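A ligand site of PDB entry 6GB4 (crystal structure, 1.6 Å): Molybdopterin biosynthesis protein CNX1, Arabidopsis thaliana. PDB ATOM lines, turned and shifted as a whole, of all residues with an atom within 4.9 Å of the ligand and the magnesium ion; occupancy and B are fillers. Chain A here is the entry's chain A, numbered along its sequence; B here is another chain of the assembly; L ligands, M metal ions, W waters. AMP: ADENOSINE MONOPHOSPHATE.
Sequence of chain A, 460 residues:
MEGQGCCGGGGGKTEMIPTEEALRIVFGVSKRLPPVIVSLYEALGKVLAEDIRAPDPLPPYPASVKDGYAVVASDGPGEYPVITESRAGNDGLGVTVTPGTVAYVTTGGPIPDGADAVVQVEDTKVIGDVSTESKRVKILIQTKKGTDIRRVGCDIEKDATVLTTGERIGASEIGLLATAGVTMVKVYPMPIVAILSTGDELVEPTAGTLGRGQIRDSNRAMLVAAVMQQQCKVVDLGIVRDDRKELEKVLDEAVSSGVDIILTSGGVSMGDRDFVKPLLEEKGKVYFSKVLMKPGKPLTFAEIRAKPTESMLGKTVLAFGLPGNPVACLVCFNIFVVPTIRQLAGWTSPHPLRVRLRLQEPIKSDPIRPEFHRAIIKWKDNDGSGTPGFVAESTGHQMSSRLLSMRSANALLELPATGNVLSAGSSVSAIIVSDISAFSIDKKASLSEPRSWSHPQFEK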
ATOM      1  N   SER A 197      -3.644  12.534 -24.775  1.00  0.00           N
ATOM      2  CA  SER A 197      -3.709  13.834 -24.087  1.00  0.00           C
ATOM      3  C   SER A 197      -3.326  14.913 -25.090  1.00  0.00           C
ATOM      4  O   SER A 197      -2.593  14.647 -26.041  1.00  0.00           O
ATOM      5  CB  SER A 197      -2.735  13.879 -22.912  1.00  0.00           C
ATOM      6  OG  SER A 197      -3.250  13.135 -21.827  1.00  0.00           O
ATOM      7  N   THR A 198      -3.780  16.130 -24.850  1.00  0.00           N
ATOM      8  CA  THR A 198      -3.387  17.245 -25.720  1.00  0.00           C
ATOM      9  C   THR A 198      -2.798  18.373 -24.910  1.00  0.00           C
ATOM     10  O   THR A 198      -3.291  18.669 -23.817  1.00  0.00           O
ATOM     11  CB  THR A 198      -4.598  17.789 -26.537  1.00  0.00           C
ATOM     12  OG1 THR A 198      -5.549  18.440 -25.682  1.00  0.00           O
ATOM     13  CG2 THR A 198      -5.274  16.699 -27.380  1.00  0.00           C
ATOM     14  N   GLY A 199      -1.798  19.059 -25.460  1.00  0.00           N
ATOM     15  CA  GLY A 199      -1.324  20.269 -24.816  1.00  0.00           C
ATOM     16  C   GLY A 199       0.137  20.555 -24.975  1.00  0.00           C
ATOM     17  O   GLY A 199       0.959  19.700 -24.645  1.00  0.00           O
ATOM     18  N   GLU A 201       1.682  22.471 -23.001  1.00  0.00           N
ATOM     19  CA  GLU A 201       2.197  22.587 -21.630  1.00  0.00           C
ATOM     20  C   GLU A 201       2.510  21.228 -20.966  1.00  0.00           C
ATOM     21  O   GLU A 201       3.104  21.201 -19.900  1.00  0.00           O
ATOM     22  CB  GLU A 201       1.254  23.420 -20.748  1.00  0.00           C
ATOM     23  CG  GLU A 201       0.007  22.712 -20.212  1.00  0.00           C
ATOM     24  CD  GLU A 201      -1.156  22.495 -21.164  1.00  0.00           C
ATOM     25  OE1 GLU A 201      -0.987  22.680 -22.391  1.00  0.00           O
ATOM     26  OE2 GLU A 201      -2.244  22.131 -20.675  1.00  0.00           O
ATOM     27  N   LEU A 202       2.123  20.108 -21.585  1.00  0.00           N
ATOM     28  CA  LEU A 202       2.311  18.797 -20.974  1.00  0.00           C
ATOM     29  C   LEU A 202       3.689  18.253 -21.170  1.00  0.00           C
ATOM     30  O   LEU A 202       4.284  18.449 -22.229  1.00  0.00           O
ATOM     31  CB  LEU A 202       1.326  17.784 -21.566  1.00  0.00           C
ATOM     32  CG  LEU A 202      -0.144  18.150 -21.509  1.00  0.00           C
ATOM     33  CD1 LEU A 202      -0.980  17.029 -22.121  1.00  0.00           C
ATOM     34  CD2 LEU A 202      -0.597  18.446 -20.064  1.00  0.00           C
ATOM     35  N   ILE A 215       3.463  21.112 -17.008  1.00  0.00           N
ATOM     36  CA  ILE A 215       2.856  20.265 -15.980  1.00  0.00           C
ATOM     37  C   ILE A 215       2.997  18.826 -16.468  1.00  0.00           C
ATOM     38  O   ILE A 215       3.059  18.602 -17.680  1.00  0.00           O
ATOM     39  CB  ILE A 215       1.369  20.578 -15.721  1.00  0.00           C
ATOM     40  CG1 ILE A 215       0.509  20.465 -17.021  1.00  0.00           C
ATOM     41  CG2 ILE A 215       1.236  21.929 -15.065  1.00  0.00           C
ATOM     42  CD1 ILE A 215      -0.961  20.454 -16.738  1.00  0.00           C
ATOM     43  N   ARG A 216       2.967  17.844 -15.567  1.00  0.00           N
ATOM     44  CA  ARG A 216       2.994  16.450 -16.019  1.00  0.00           C
ATOM     45  C   ARG A 216       1.623  16.075 -16.535  1.00  0.00           C
ATOM     46  O   ARG A 216       0.590  16.491 -15.982  1.00  0.00           O
ATOM     47  CB  ARG A 216       3.326  15.483 -14.842  1.00  0.00           C
ATOM     48  CG  ARG A 216       4.779  15.697 -14.352  1.00  0.00           C
ATOM     49  CD  ARG A 216       5.275  14.726 -13.255  1.00  0.00           C
ATOM     50  NE  ARG A 216       6.576  15.218 -12.762  1.00  0.00           N
ATOM     51  CZ  ARG A 216       6.723  16.155 -11.823  1.00  0.00           C
ATOM     52  NH1 ARG A 216       5.660  16.655 -11.201  1.00  0.00           N
ATOM     53  NH2 ARG A 216       7.932  16.623 -11.525  1.00  0.00           N
ATOM     54  N   ASP A 217       1.594  15.253 -17.580  1.00  0.00           N
ATOM     55  CA  ASP A 217       0.351  14.722 -18.132  1.00  0.00           C
ATOM     56  C   ASP A 217      -0.203  13.731 -17.072  1.00  0.00           C
ATOM     57  O   ASP A 217       0.385  12.664 -16.873  1.00  0.00           O
ATOM     58  CB  ASP A 217       0.681  13.955 -19.423  1.00  0.00           C
ATOM     59  CG  ASP A 217      -0.439  13.233 -20.120  1.00  0.00           C
ATOM     60  OD1 ASP A 217      -1.600  13.387 -19.704  1.00  0.00           O
ATOM     61  OD2 ASP A 217      -0.162  12.546 -21.107  1.00  0.00           O
ATOM     62  N   SER A 218      -1.288  14.108 -16.389  1.00  0.00           N
ATOM     63  CA  SER A 218      -1.934  13.203 -15.414  1.00  0.00           C
ATOM     64  C   SER A 218      -3.228  12.569 -15.991  1.00  0.00           C
ATOM     65  O   SER A 218      -3.576  11.442 -15.583  1.00  0.00           O
ATOM     66  CB  SER A 218      -2.238  13.942 -14.108  1.00  0.00           C
ATOM     67  OG  SER A 218      -3.161  15.000 -14.306  1.00  0.00           O
ATOM     68  N   ASN A 219      -3.930  13.226 -16.943  1.00  0.00           N
ATOM     69  CA  ASN A 219      -5.193  12.687 -17.445  1.00  0.00           C
ATOM     70  C   ASN A 219      -5.018  11.367 -18.152  1.00  0.00           C
ATOM     71  O   ASN A 219      -5.872  10.507 -18.044  1.00  0.00           O
ATOM     72  CB  ASN A 219      -5.873  13.654 -18.413  1.00  0.00           C
ATOM     73  CG  ASN A 219      -6.453  14.864 -17.754  1.00  0.00           C
ATOM     74  OD1 ASN A 219      -6.554  14.932 -16.534  1.00  0.00           O
ATOM     75  ND2 ASN A 219      -6.852  15.875 -18.534  1.00  0.00           N
ATOM     76  N   ARG A 220      -3.948  11.242 -18.918  1.00  0.00           N
ATOM     77  CA  ARG A 220      -3.764  10.035 -19.716  1.00  0.00           C
ATOM     78  C   ARG A 220      -3.612   8.795 -18.825  1.00  0.00           C
ATOM     79  O   ARG A 220      -4.390   7.851 -18.990  1.00  0.00           O
ATOM     80  CB  ARG A 220      -2.563  10.181 -20.665  1.00  0.00           C
ATOM     81  CG  ARG A 220      -2.386   9.007 -21.651  1.00  0.00           C
ATOM     82  CD  ARG A 220      -1.583   9.431 -22.853  1.00  0.00           C
ATOM     83  NE  ARG A 220      -0.403  10.182 -22.428  1.00  0.00           N
ATOM     84  CZ  ARG A 220       0.818   9.713 -22.223  1.00  0.00           C
ATOM     85  NH1 ARG A 220       1.127   8.459 -22.562  1.00  0.00           N
ATOM     86  NH2 ARG A 220       1.764  10.508 -21.764  1.00  0.00           N
ATOM     87  N   ASP A 242      -0.720  21.110 -29.477  1.00  0.00           N
ATOM     88  CA  ASP A 242      -1.813  21.980 -29.945  1.00  0.00           C
ATOM     89  C   ASP A 242      -1.515  22.447 -31.365  1.00  0.00           C
ATOM     90  O   ASP A 242      -1.249  23.624 -31.611  1.00  0.00           O
ATOM     91  CB  ASP A 242      -1.988  23.144 -28.950  1.00  0.00           C
ATOM     92  CG  ASP A 242      -2.365  22.647 -27.565  1.00  0.00           C
ATOM     93  OD1 ASP A 242      -3.185  21.677 -27.470  1.00  0.00           O
ATOM     94  OD2 ASP A 242      -1.840  23.202 -26.567  1.00  0.00           O
ATOM     95  N   SER A 265      -8.373  14.243 -24.139  1.00  0.00           N
ATOM     96  CA  SER A 265      -8.697  15.232 -23.096  1.00  0.00           C
ATOM     97  C   SER A 265      -8.019  16.538 -23.457  1.00  0.00           C
ATOM     98  O   SER A 265      -7.004  16.550 -24.132  1.00  0.00           O
ATOM     99  CB  SER A 265      -8.336  14.788 -21.682  1.00  0.00           C
ATOM    100  OG  SER A 265      -6.931  14.817 -21.427  1.00  0.00           O
ATOM    101  N   GLY A 266      -8.622  17.640 -23.028  1.00  0.00           N
ATOM    102  CA  GLY A 266      -8.079  18.951 -23.305  1.00  0.00           C
ATOM    103  C   GLY A 266      -8.386  19.397 -24.719  1.00  0.00           C
ATOM    104  O   GLY A 266      -8.996  18.646 -25.483  1.00  0.00           O
ATOM    105  N   GLY A 267      -7.948  20.594 -25.085  1.00  0.00           N
ATOM    106  CA  GLY A 267      -8.144  21.083 -26.449  1.00  0.00           C
ATOM    107  C   GLY A 267      -9.588  21.350 -26.827  1.00  0.00           C
ATOM    108  O   GLY A 267      -9.901  21.443 -28.020  1.00  0.00           O
ATOM    109  N   VAL A 268     -10.480  21.466 -25.819  1.00  0.00           N
ATOM    110  CA  VAL A 268     -11.922  21.703 -26.018  1.00  0.00           C
ATOM    111  C   VAL A 268     -12.377  22.990 -25.327  1.00  0.00           C
ATOM    112  O   VAL A 268     -13.584  23.153 -25.136  1.00  0.00           O
ATOM    113  CB  VAL A 268     -12.797  20.475 -25.595  1.00  0.00           C
ATOM    114  CG1 VAL A 268     -12.638  19.317 -26.579  1.00  0.00           C
ATOM    115  CG2 VAL A 268     -12.484  20.028 -24.173  1.00  0.00           C
ATOM    116  N   SER A 269     -11.467  23.905 -24.952  1.00  0.00           N
ATOM    117  CA  SER A 269     -11.894  25.183 -24.343  1.00  0.00           C
ATOM    118  C   SER A 269     -12.062  26.236 -25.477  1.00  0.00           C
ATOM    119  O   SER A 269     -12.326  25.858 -26.625  1.00  0.00           O
ATOM    120  CB  SER A 269     -10.901  25.627 -23.258  1.00  0.00           C
ATOM    121  OG  SER A 269     -10.684  24.631 -22.286  1.00  0.00           O
ATOM    122  N   ASP A 274      -7.279  25.270 -29.749  1.00  0.00           N
ATOM    123  CA  ASP A 274      -8.134  24.160 -29.265  1.00  0.00           C
ATOM    124  C   ASP A 274      -8.786  23.594 -30.530  1.00  0.00           C
ATOM    125  O   ASP A 274      -9.661  24.246 -31.091  1.00  0.00           O
ATOM    126  CB  ASP A 274      -9.173  24.681 -28.253  1.00  0.00           C
ATOM    127  CG  ASP A 274      -8.584  24.931 -26.882  1.00  0.00           C
ATOM    128  OD1 ASP A 274      -7.533  24.365 -26.581  1.00  0.00           O
ATOM    129  OD2 ASP A 274      -9.152  25.722 -26.133  1.00  0.00           O
ATOM    130  N   PRO A 323     -13.036  17.099 -21.192  1.00  0.00           N
ATOM    131  CA  PRO A 323     -12.396  18.351 -20.759  1.00  0.00           C
ATOM    132  C   PRO A 323     -10.995  18.087 -20.228  1.00  0.00           C
ATOM    133  O   PRO A 323     -10.721  16.998 -19.725  1.00  0.00           O
ATOM    134  CB  PRO A 323     -13.323  18.899 -19.651  1.00  0.00           C
ATOM    135  CG  PRO A 323     -14.337  17.855 -19.417  1.00  0.00           C
ATOM    136  CD  PRO A 323     -14.258  16.787 -20.419  1.00  0.00           C
ATOM    137  N   GLY A 324     -10.121  19.086 -20.357  1.00  0.00           N
ATOM    138  CA  GLY A 324      -8.745  18.954 -19.866  1.00  0.00           C
ATOM    139  C   GLY A 324      -8.633  19.028 -18.352  1.00  0.00           C
ATOM    140  O   GLY A 324      -7.725  18.442 -17.769  1.00  0.00           O
ATOM    141  N   ASN A 325      -9.516  19.792 -17.668  1.00  0.00           N
ATOM    142  CA  ASN A 325      -9.376  19.883 -16.196  1.00  0.00           C
ATOM    143  C   ASN A 325      -9.474  18.494 -15.565  1.00  0.00           C
ATOM    144  O   ASN A 325     -10.435  17.789 -15.868  1.00  0.00           O
ATOM    145  CB  ASN A 325     -10.399  20.813 -15.602  1.00  0.00           C
ATOM    146  CG  ASN A 325      -9.949  22.272 -15.650  1.00  0.00           C
ATOM    147  OD1 ASN A 325      -8.944  22.660 -15.046  1.00  0.00           O
ATOM    148  ND2 ASN A 325     -10.662  23.091 -16.380  1.00  0.00           N
ATOM    149  N   PRO A 326      -8.474  18.031 -14.775  1.00  0.00           N
ATOM    150  CA  PRO A 326      -8.500  16.620 -14.282  1.00  0.00           C
ATOM    151  C   PRO A 326      -9.805  16.144 -13.679  1.00  0.00           C
ATOM    152  O   PRO A 326     -10.243  15.045 -13.954  1.00  0.00           O
ATOM    153  CB  PRO A 326      -7.373  16.615 -13.246  1.00  0.00           C
ATOM    154  CG  PRO A 326      -6.335  17.515 -13.857  1.00  0.00           C
ATOM    155  CD  PRO A 326      -7.180  18.667 -14.431  1.00  0.00           C
ATOM    156  N   SER B  64      -3.557  30.512 -15.965  1.00  0.00           N
ATOM    157  CA  SER B  64      -4.849  31.063 -16.294  1.00  0.00           C
ATOM    158  C   SER B  64      -5.930  29.981 -16.213  1.00  0.00           C
ATOM    159  O   SER B  64      -5.742  28.866 -16.708  1.00  0.00           O
ATOM    160  CB  SER B  64      -4.852  31.626 -17.712  1.00  0.00           C
ATOM    161  OG  SER B  64      -6.125  32.159 -17.970  1.00  0.00           O
ATOM    162  N   THR B 107      -6.288  28.672 -21.442  1.00  0.00           N
ATOM    163  CA  THR B 107      -6.439  27.940 -20.181  1.00  0.00           C
ATOM    164  C   THR B 107      -5.182  27.145 -19.929  1.00  0.00           C
ATOM    165  O   THR B 107      -4.650  26.536 -20.853  1.00  0.00           O
ATOM    166  CB  THR B 107      -7.712  27.052 -20.189  1.00  0.00           C
ATOM    167  OG1 THR B 107      -8.827  27.826 -20.629  1.00  0.00           O
ATOM    168  CG2 THR B 107      -8.030  26.481 -18.804  1.00  0.00           C
ATOM    169  N   GLY B 108      -4.655  27.257 -18.715  1.00  0.00           N
ATOM    170  CA  GLY B 108      -3.410  26.611 -18.339  1.00  0.00           C
ATOM    171  C   GLY B 108      -2.173  27.381 -18.750  1.00  0.00           C
ATOM    172  O   GLY B 108      -1.065  26.959 -18.424  1.00  0.00           O
ATOM    173  N   ARG B 150      -4.995  30.625 -11.233  1.00  0.00           N
ATOM    174  CA  ARG B 150      -4.646  29.594 -10.260  1.00  0.00           C
ATOM    175  C   ARG B 150      -3.261  29.950  -9.768  1.00  0.00           C
ATOM    176  O   ARG B 150      -2.308  29.811 -10.540  1.00  0.00           O
ATOM    177  CB  ARG B 150      -4.627  28.197 -10.916  1.00  0.00           C
ATOM    178  CG  ARG B 150      -6.023  27.640 -11.178  1.00  0.00           C
ATOM    179  CD  ARG B 150      -5.996  26.561 -12.243  1.00  0.00           C
ATOM    180  NE  ARG B 150      -5.174  25.420 -11.812  1.00  0.00           N
ATOM    181  CZ  ARG B 150      -4.287  24.753 -12.550  1.00  0.00           C
ATOM    182  NH1 ARG B 150      -4.085  25.081 -13.820  1.00  0.00           N
ATOM    183  NH2 ARG B 150      -3.589  23.754 -12.015  1.00  0.00           N
HETATM  184  P   AMP L   1      -7.713  22.514 -22.042  1.00  0.00           P
HETATM  185  O1P AMP L   1      -7.962  23.992 -22.198  1.00  0.00           O
HETATM  186  O2P AMP L   1      -6.644  22.000 -23.001  1.00  0.00           O
HETATM  187  O3P AMP L   1      -8.993  21.748 -21.956  1.00  0.00           O
HETATM  188  O5' AMP L   1      -7.179  22.394 -20.541  1.00  0.00           O
HETATM  189  C5' AMP L   1      -7.942  22.813 -19.403  1.00  0.00           C
HETATM  190  C4' AMP L   1      -7.039  22.755 -18.154  1.00  0.00           C
HETATM  191  O4' AMP L   1      -6.698  21.358 -17.943  1.00  0.00           O
HETATM  192  C3' AMP L   1      -5.713  23.478 -18.278  1.00  0.00           C
HETATM  193  O3' AMP L   1      -5.348  24.030 -16.996  1.00  0.00           O
HETATM  194  C2' AMP L   1      -4.741  22.395 -18.706  1.00  0.00           C
HETATM  195  O2' AMP L   1      -3.368  22.677 -18.398  1.00  0.00           O
HETATM  196  C1' AMP L   1      -5.285  21.191 -17.948  1.00  0.00           C
HETATM  197  N9  AMP L   1      -4.937  19.918 -18.648  1.00  0.00           N
HETATM  198  C8  AMP L   1      -5.185  19.621 -19.945  1.00  0.00           C
HETATM  199  N7  AMP L   1      -4.749  18.381 -20.248  1.00  0.00           N
HETATM  200  C5  AMP L   1      -4.215  17.871 -19.112  1.00  0.00           C
HETATM  201  C6  AMP L   1      -3.548  16.603 -18.758  1.00  0.00           C
HETATM  202  N6  AMP L   1      -3.419  15.655 -19.696  1.00  0.00           N
HETATM  203  N1  AMP L   1      -3.147  16.438 -17.475  1.00  0.00           N
HETATM  204  C2  AMP L   1      -3.302  17.395 -16.543  1.00  0.00           C
HETATM  205  N3  AMP L   1      -3.897  18.585 -16.808  1.00  0.00           N
HETATM  206  C4  AMP L   1      -4.357  18.873 -18.048  1.00  0.00           C
HETATM  207 MG    MG M   1      -4.870  22.503 -23.599  1.00  0.00          MG
HETATM  208  O   HOH W   1      -3.475  19.745 -14.245  1.00  0.00           O
HETATM  209  O   HOH W   2     -11.445  21.797 -21.333  1.00  0.00           O
HETATM  210  O   HOH W   3      -2.162  23.982 -16.048  1.00  0.00           O
HETATM  211  O   HOH W   4      -5.713  24.022 -24.794  1.00  0.00           O
HETATM  212  O   HOH W   5      -4.910  21.231 -25.254  1.00  0.00           O
HETATM  213  O   HOH W   6      -4.641  23.771 -21.955  1.00  0.00           O
HETATM  214  O   HOH W   7      -6.257  22.514 -14.876  1.00  0.00           O
HETATM  215  O   HOH W   8      -6.093  26.247 -15.711  1.00  0.00           O
HETATM  216  O   HOH W   9      -3.086  23.262 -24.089  1.00  0.00           O
HETATM  217  O   HOH W  10      -3.913  21.063 -22.475  1.00  0.00           O
HETATM  218  O   HOH W  11      -4.810  16.289 -22.180  1.00  0.00           O
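N of Ser 218 is in hydrogen-bond range of N1 of the ligand (3.2 Å). The backbone NH (N) of Asn 325 is in hydrogen-bond range of an oxygen (O4') of the ligand, 3.2 Å away. The backbone NH (N) of Gly 267 sits at hydrogen-bond distance from an oxygen (O3P) of the ligand (3.5 Å). An oxygen (O2') of the ligand is in hydrogen-bond range of the side-chain carboxylate (OE2) of Glu 201, 2.6 Å away. OG of Ser 218 sits close to N1 of the ligand, at 3.5 Å. The side-chain hydroxyl of Ser 197 lies within hydrogen-bond range of a nitrogen (N6) of the ligand, at 3.3 Å. N1 of the ligand is in hydrogen-bond range of N of Asn 219 (3.3 Å). O1P of the ligand sits at hydrogen-bond distance from OG of Ser 269 (2.8 Å). O3P of the ligand sits at hydrogen-bond distance from N of Gly 324 (3.3 Å). A nitrogen (N6) of the ligand lies within hydrogen-bond range of the side-chain carboxylate (OD1) of Asp 217 (2.9 Å).
The backbone NH (N) of Ser 269 sits close to the side-chain carboxylate (OD2) of Asp 274 (3.2 Å). OD2 of Asp 217 is in salt-bridge range of NE of Arg 220 (2.7 Å). The backbone NH of Gly 108 of chain B is in hydrogen-bond range of the backbone carbonyl oxygen of Ser 64 of chain B, at 2.8 Å. The backbone carbonyl oxygen of Gly 324 lies within hydrogen-bond range of the side-chain amide nitrogen of Asn 219, at 2.8 Å. The side-chain amide nitrogen (ND2) of Asn 219 sits at hydrogen-bond distance from the side-chain hydroxyl (OG) of Ser 265 (3.1 Å). OD1 of Asp 217 lies within hydrogen-bond range of OG of Ser 197 (2.7 Å). O of Glu 201 lies within hydrogen-bond range of N of Ile 215 (2.9 Å). The backbone NH (N) of Gly 267 sits at hydrogen-bond distance from the side-chain hydroxyl (OG1) of Thr 198 (3.3 Å).
O of Thr 198 touches N7 of the ligand, 3.9 Å away. Leu 202 touches the ligand (CD1 to N6, 3.7 Å). Ile 215 touches the ligand (CD1 to N3, 3.5 Å). Gly 266 touches the ligand. CG of Pro 326 touches N3 of the ligand, at 3.97 Å. CB of Thr 107 of chain B touches O1P of the ligand, 3.7 Å away. Gly 108 of chain B touches the ligand (CA to O3', 3.5 Å). Arg 150 of chain B touches the ligand (NH1 to O3', 3.6 Å). 17 residues have an atom within 4 Å of the ligand: Ser 197, Thr 198, Glu 201, Leu 202, Ile 215, Asp 217, Ser 218, Asn 219, Gly 266, Gly 267, Ser 269, Gly 324, Asn 325, Pro 326, Thr 107 of chain B, Gly 108 of chain B and Arg 150 of chain B.
Merely in contact with the magnesium ion: Glu 201 (3.9 Å) and Gly 267 (3.9 Å). Of the 26 residues printed, 2 come within 4 Å of the magnesium ion. The nearest printed residue that does not touch the magnesium ion is Thr 198 (4.2 Å).
An oxygen (O2P) of the ligand is bound to the magnesium ion (1.9 Å). The magnesium ion is bound by water W9 (2.0 Å). The magnesium ion is bound by water W10 (2.1 Å). Water W5 binds the magnesium ion (2.1 Å). Water W6 binds the magnesium ion (2.1 Å). The magnesium ion is bound by water W4 (2.1 Å). The magnesium ion has six donor atoms within binding distance.
Water W4 bridges OD1 of Asp 274 (2.6 Å) and O1P of the ligand (3.4 Å). Water W10 bridges OE2 of Glu 201 and O of Thr 198. Water W2 lies within hydrogen-bond range of an oxygen (O3P) of the ligand (2.5 Å), the side-chain hydroxyl of Ser 269 (3.1 Å) and the backbone NH of Gly 324 (3.2 Å). Water W8 lies within hydrogen-bond range of O3' of the ligand (2.7 Å), O of Ser 64 of chain B (2.8 Å), NH1 of Arg 150 of chain B (3.0 Å) and N of Gly 108 of chain B (3.5 Å). Water W11 lies within hydrogen-bond range of the side-chain hydroxyl (OG) of Ser 265 (2.7 Å), a nitrogen (N7) of the ligand (2.8 Å) and the backbone NH (N) of Thr 198 (2.9 Å). Water W3 bridges O2' of the ligand (2.9 Å) and NH1 of Arg 150 of chain B (3.1 Å).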
